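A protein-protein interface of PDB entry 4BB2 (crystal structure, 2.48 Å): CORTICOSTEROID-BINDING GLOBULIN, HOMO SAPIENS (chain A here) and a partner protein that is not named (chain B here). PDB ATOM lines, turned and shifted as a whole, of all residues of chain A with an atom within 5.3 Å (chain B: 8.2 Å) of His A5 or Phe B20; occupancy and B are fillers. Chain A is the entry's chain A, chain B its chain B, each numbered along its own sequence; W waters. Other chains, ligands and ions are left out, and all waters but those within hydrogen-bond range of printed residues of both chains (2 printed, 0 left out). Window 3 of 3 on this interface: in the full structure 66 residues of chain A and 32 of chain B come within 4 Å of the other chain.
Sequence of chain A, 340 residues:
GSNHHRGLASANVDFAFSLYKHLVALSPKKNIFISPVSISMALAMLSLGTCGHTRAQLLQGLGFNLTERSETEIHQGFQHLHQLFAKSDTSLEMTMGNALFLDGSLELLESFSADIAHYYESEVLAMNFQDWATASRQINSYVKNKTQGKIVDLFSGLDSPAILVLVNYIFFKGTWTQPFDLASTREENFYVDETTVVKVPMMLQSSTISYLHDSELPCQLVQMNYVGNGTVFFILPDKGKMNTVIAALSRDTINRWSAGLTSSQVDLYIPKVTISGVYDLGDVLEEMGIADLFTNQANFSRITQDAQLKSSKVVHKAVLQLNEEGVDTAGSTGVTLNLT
O of Phe B20 lies within hydrogen-bond range of NE of Arg A6. N of His B19 lies close to O of Asn A229, at 3.1 Å. The guanidinium group (NH2) of Arg A6 lies within hydrogen-bond range of the backbone carbonyl oxygen (O) of His B19.
O of Ser B23 lies within hydrogen-bond range of N of Asp B18 (3.1 Å). OG1 of Thr B21 sits at hydrogen-bond distance from OG of Ser B23 (2.8 Å). OD2 of Asp B18 lies within hydrogen-bond range of OG1 of Thr B21 (2.7 Å). OD1 of Asp B18 is in hydrogen-bond range of N of Phe B20, at 2.9 Å.
His A5 touches Phe B20. CB of Thr B21 touches O of His A5, at 3.6 Å. Thr B21 touches Arg A6. Arg A6 touches Trp B22. Thr B21 touches Leu A81 (CG2 to CD2, 3.6 Å). CD2 of Leu A81 touches OG of Ser B23 (3.8 Å). Phe B20 touches Leu A84. Leu A84 touches Thr B21 (CD1 to CG2, 3.6 Å). CB of Asn A229 touches OD1 of Asp B18, 3.4 Å away.
Of chain B, only Phe B20 and Thr B21 come within 4 Å of His A5. Of the printed residues of chain A, Thr B21 touches His A5, Arg A6, Leu A81 and Leu A84. Of the printed residues of chain A, Trp B22 touches Arg A6 (3.3 Å). Of the printed residues of chain A, Asp B18 touches Asn A229. Printed residues of chain B within 4 Å of Leu A81: Thr B21 and Ser B23. His A4 touches none of the printed residues of chain B. Phe B17 touches none of the printed residues of chain A. The nearest residue of chain B that does not touch His A5 is Trp B22 (5.9 Å).
Of the 7 printed residues of chain B, 6 touch a printed residue of chain A. Printed residues of chain B that touch a printed residue of chain A: Asp B18, His B19, Phe B20, Thr B21, Trp B22 and Ser B23. Hydrophobic or aromatic side chains of chain B within 4 Å of the printed part of chain A: His B19, Phe B20 and Trp B22. Printed residues of chain A that touch a printed residue of chain B: His A5, Arg A6, Leu A81, Leu A84 and Asn A229. Hydrophobic or aromatic side chains of chain A that line the printed part of chain B: His A5, Leu A81 and Leu A84. Among the printed residues, 12 pairs touch across the chains. Among the printed residues, no Asp or Glu carboxylate lies within 4 Å of a Lys or Arg side-chain nitrogen of the other chain.
Water W1 bridges NE2 of His B19 (2.9 Å) and NH2 of Arg A6 (3.1 Å). Water W2 lies within hydrogen-bond range of the side-chain amide nitrogen of Asn A229 and the side-chain carboxylate of Asp B18.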
ATOM      1  N   HIS A   4      10.187   6.529 -22.178  1.00  0.00           N
ATOM      2  CA  HIS A   4      10.379   7.995 -22.359  1.00  0.00           C
ATOM      3  C   HIS A   4      10.855   8.631 -21.052  1.00  0.00           C
ATOM      4  O   HIS A   4      10.278   8.390 -19.988  1.00  0.00           O
ATOM      5  CB  HIS A   4       9.090   8.636 -22.899  1.00  0.00           C
ATOM      6  CG  HIS A   4       8.963  10.106 -22.626  1.00  0.00           C
ATOM      7  ND1 HIS A   4       9.762  11.051 -23.235  1.00  0.00           N
ATOM      8  CD2 HIS A   4       8.110  10.791 -21.830  1.00  0.00           C
ATOM      9  CE1 HIS A   4       9.413  12.254 -22.816  1.00  0.00           C
ATOM     10  NE2 HIS A   4       8.414  12.123 -21.961  1.00  0.00           N
ATOM     11  N   HIS A   5      11.908   9.448 -21.150  1.00  0.00           N
ATOM     12  CA  HIS A   5      12.653   9.930 -19.980  1.00  0.00           C
ATOM     13  C   HIS A   5      12.169  11.281 -19.413  1.00  0.00           C
ATOM     14  O   HIS A   5      11.484  11.309 -18.383  1.00  0.00           O
ATOM     15  CB  HIS A   5      14.170   9.964 -20.267  1.00  0.00           C
ATOM     16  CG  HIS A   5      14.631   8.937 -21.261  1.00  0.00           C
ATOM     17  ND1 HIS A   5      14.389   7.586 -21.113  1.00  0.00           N
ATOM     18  CD2 HIS A   5      15.324   9.067 -22.419  1.00  0.00           C
ATOM     19  CE1 HIS A   5      14.908   6.930 -22.137  1.00  0.00           C
ATOM     20  NE2 HIS A   5      15.480   7.806 -22.945  1.00  0.00           N
ATOM     21  N   ARG A   6      12.503  12.380 -20.095  1.00  0.00           N
ATOM     22  CA  ARG A   6      12.471  13.732 -19.500  1.00  0.00           C
ATOM     23  C   ARG A   6      11.348  14.698 -19.920  1.00  0.00           C
ATOM     24  O   ARG A   6      11.411  15.889 -19.604  1.00  0.00           O
ATOM     25  CB  ARG A   6      13.830  14.414 -19.707  1.00  0.00           C
ATOM     26  CG  ARG A   6      14.964  13.775 -18.929  1.00  0.00           C
ATOM     27  CD  ARG A   6      16.318  14.143 -19.513  1.00  0.00           C
ATOM     28  NE  ARG A   6      17.406  13.613 -18.694  1.00  0.00           N
ATOM     29  CZ  ARG A   6      18.670  13.496 -19.092  1.00  0.00           C
ATOM     30  NH1 ARG A   6      19.027  13.877 -20.313  1.00  0.00           N
ATOM     31  NH2 ARG A   6      19.581  12.991 -18.264  1.00  0.00           N
ATOM     32  N   GLY A   7      10.321  14.191 -20.599  1.00  0.00           N
ATOM     33  CA  GLY A   7       9.249  15.030 -21.154  1.00  0.00           C
ATOM     34  C   GLY A   7       8.515  15.961 -20.202  1.00  0.00           C
ATOM     35  O   GLY A   7       8.147  17.075 -20.573  1.00  0.00           O
ATOM     36  N   LEU A  81       7.180   7.547 -16.784  1.00  0.00           N
ATOM     37  CA  LEU A  81       7.793   7.726 -15.479  1.00  0.00           C
ATOM     38  C   LEU A  81       7.584   6.493 -14.601  1.00  0.00           C
ATOM     39  O   LEU A  81       8.539   5.915 -14.075  1.00  0.00           O
ATOM     40  CB  LEU A  81       7.218   8.951 -14.772  1.00  0.00           C
ATOM     41  CG  LEU A  81       7.903  10.308 -14.912  1.00  0.00           C
ATOM     42  CD1 LEU A  81       7.563  11.158 -13.692  1.00  0.00           C
ATOM     43  CD2 LEU A  81       9.412  10.183 -15.061  1.00  0.00           C
ATOM     44  N   LEU A  84       9.540   3.390 -15.599  1.00  0.00           N
ATOM     45  CA  LEU A  84      10.953   3.532 -15.261  1.00  0.00           C
ATOM     46  C   LEU A  84      11.266   3.311 -13.784  1.00  0.00           C
ATOM     47  O   LEU A  84      12.298   2.730 -13.457  1.00  0.00           O
ATOM     48  CB  LEU A  84      11.504   4.878 -15.722  1.00  0.00           C
ATOM     49  CG  LEU A  84      11.757   4.995 -17.225  1.00  0.00           C
ATOM     50  CD1 LEU A  84      12.239   6.396 -17.569  1.00  0.00           C
ATOM     51  CD2 LEU A  84      12.754   3.954 -17.714  1.00  0.00           C
ATOM     52  N   ASN A 229      21.190   5.833 -10.340  1.00  0.00           N
ATOM     53  CA  ASN A 229      20.880   7.114 -10.996  1.00  0.00           C
ATOM     54  C   ASN A 229      20.600   8.280 -10.045  1.00  0.00           C
ATOM     55  O   ASN A 229      20.680   9.437 -10.447  1.00  0.00           O
ATOM     56  CB  ASN A 229      19.744   6.959 -12.024  1.00  0.00           C
ATOM     57  CG  ASN A 229      20.126   6.059 -13.198  1.00  0.00           C
ATOM     58  OD1 ASN A 229      21.173   6.240 -13.823  1.00  0.00           O
ATOM     59  ND2 ASN A 229      19.264   5.096 -13.515  1.00  0.00           N
ATOM     60  N   PHE B  17      17.190  14.027  -6.625  1.00  0.00           N
ATOM     61  CA  PHE B  17      16.784  13.911  -8.026  1.00  0.00           C
ATOM     62  C   PHE B  17      17.158  12.565  -8.630  1.00  0.00           C
ATOM     63  O   PHE B  17      18.186  11.976  -8.284  1.00  0.00           O
ATOM     64  CB  PHE B  17      17.425  15.017  -8.894  1.00  0.00           C
ATOM     65  CG  PHE B  17      16.907  16.395  -8.617  1.00  0.00           C
ATOM     66  CD1 PHE B  17      15.805  16.892  -9.300  1.00  0.00           C
ATOM     67  CD2 PHE B  17      17.523  17.211  -7.678  1.00  0.00           C
ATOM     68  CE1 PHE B  17      15.326  18.175  -9.048  1.00  0.00           C
ATOM     69  CE2 PHE B  17      17.044  18.489  -7.416  1.00  0.00           C
ATOM     70  CZ  PHE B  17      15.946  18.974  -8.107  1.00  0.00           C
ATOM     71  N   ASP B  18      16.319  12.106  -9.555  1.00  0.00           N
ATOM     72  CA  ASP B  18      16.684  11.046 -10.474  1.00  0.00           C
ATOM     73  C   ASP B  18      17.395  11.669 -11.668  1.00  0.00           C
ATOM     74  O   ASP B  18      16.763  12.321 -12.499  1.00  0.00           O
ATOM     75  CB  ASP B  18      15.439  10.276 -10.936  1.00  0.00           C
ATOM     76  CG  ASP B  18      15.722   9.341 -12.110  1.00  0.00           C
ATOM     77  OD1 ASP B  18      16.845   8.809 -12.235  1.00  0.00           O
ATOM     78  OD2 ASP B  18      14.805   9.130 -12.914  1.00  0.00           O
ATOM     79  N   HIS B  19      18.709  11.457 -11.743  1.00  0.00           N
ATOM     80  CA  HIS B  19      19.548  11.896 -12.865  1.00  0.00           C
ATOM     81  C   HIS B  19      18.999  11.448 -14.225  1.00  0.00           C
ATOM     82  O   HIS B  19      19.198  12.132 -15.233  1.00  0.00           O
ATOM     83  CB  HIS B  19      20.970  11.346 -12.685  1.00  0.00           C
ATOM     84  CG  HIS B  19      22.017  12.050 -13.494  1.00  0.00           C
ATOM     85  ND1 HIS B  19      23.056  12.750 -12.914  1.00  0.00           N
ATOM     86  CD2 HIS B  19      22.209  12.139 -14.832  1.00  0.00           C
ATOM     87  CE1 HIS B  19      23.840  13.239 -13.859  1.00  0.00           C
ATOM     88  NE2 HIS B  19      23.343  12.892 -15.032  1.00  0.00           N
ATOM     89  N   PHE B  20      18.313  10.307 -14.259  1.00  0.00           N
ATOM     90  CA  PHE B  20      17.799   9.774 -15.521  1.00  0.00           C
ATOM     91  C   PHE B  20      16.592  10.554 -16.054  1.00  0.00           C
ATOM     92  O   PHE B  20      16.620  11.037 -17.185  1.00  0.00           O
ATOM     93  CB  PHE B  20      17.486   8.280 -15.401  1.00  0.00           C
ATOM     94  CG  PHE B  20      17.377   7.577 -16.722  1.00  0.00           C
ATOM     95  CD1 PHE B  20      18.521   7.256 -17.452  1.00  0.00           C
ATOM     96  CD2 PHE B  20      16.131   7.229 -17.240  1.00  0.00           C
ATOM     97  CE1 PHE B  20      18.422   6.600 -18.675  1.00  0.00           C
ATOM     98  CE2 PHE B  20      16.024   6.568 -18.463  1.00  0.00           C
ATOM     99  CZ  PHE B  20      17.169   6.258 -19.182  1.00  0.00           C
ATOM    100  N   THR B  21      15.539  10.684 -15.252  1.00  0.00           N
ATOM    101  CA  THR B  21      14.360  11.449 -15.675  1.00  0.00           C
ATOM    102  C   THR B  21      14.366  12.908 -15.238  1.00  0.00           C
ATOM    103  O   THR B  21      13.551  13.693 -15.727  1.00  0.00           O
ATOM    104  CB  THR B  21      13.038  10.839 -15.173  1.00  0.00           C
ATOM    105  OG1 THR B  21      12.958  10.958 -13.746  1.00  0.00           O
ATOM    106  CG2 THR B  21      12.908   9.391 -15.603  1.00  0.00           C
ATOM    107  N   TRP B  22      15.271  13.258 -14.324  1.00  0.00           N
ATOM    108  CA  TRP B  22      15.326  14.589 -13.712  1.00  0.00           C
ATOM    109  C   TRP B  22      14.174  14.860 -12.737  1.00  0.00           C
ATOM    110  O   TRP B  22      13.923  16.011 -12.387  1.00  0.00           O
ATOM    111  CB  TRP B  22      15.374  15.698 -14.765  1.00  0.00           C
ATOM    112  CG  TRP B  22      16.671  15.829 -15.511  1.00  0.00           C
ATOM    113  CD1 TRP B  22      17.907  15.386 -15.116  1.00  0.00           C
ATOM    114  CD2 TRP B  22      16.866  16.505 -16.762  1.00  0.00           C
ATOM    115  NE1 TRP B  22      18.854  15.721 -16.062  1.00  0.00           N
ATOM    116  CE2 TRP B  22      18.244  16.407 -17.081  1.00  0.00           C
ATOM    117  CE3 TRP B  22      16.007  17.174 -17.654  1.00  0.00           C
ATOM    118  CZ2 TRP B  22      18.784  16.957 -18.259  1.00  0.00           C
ATOM    119  CZ3 TRP B  22      16.547  17.715 -18.829  1.00  0.00           C
ATOM    120  CH2 TRP B  22      17.923  17.604 -19.117  1.00  0.00           C
ATOM    121  N   SER B  23      13.486  13.808 -12.295  1.00  0.00           N
ATOM    122  CA  SER B  23      12.398  13.939 -11.335  1.00  0.00           C
ATOM    123  C   SER B  23      12.884  14.522 -10.017  1.00  0.00           C
ATOM    124  O   SER B  23      13.983  14.199  -9.539  1.00  0.00           O
ATOM    125  CB  SER B  23      11.763  12.575 -11.034  1.00  0.00           C
ATOM    126  OG  SER B  23      11.014  12.066 -12.118  1.00  0.00           O
HETATM  127  O   HOH W   1      22.025  14.532 -17.047  1.00  0.00           O
HETATM  128  O   HOH W   2      16.216   5.712 -13.567  1.00  0.00           O
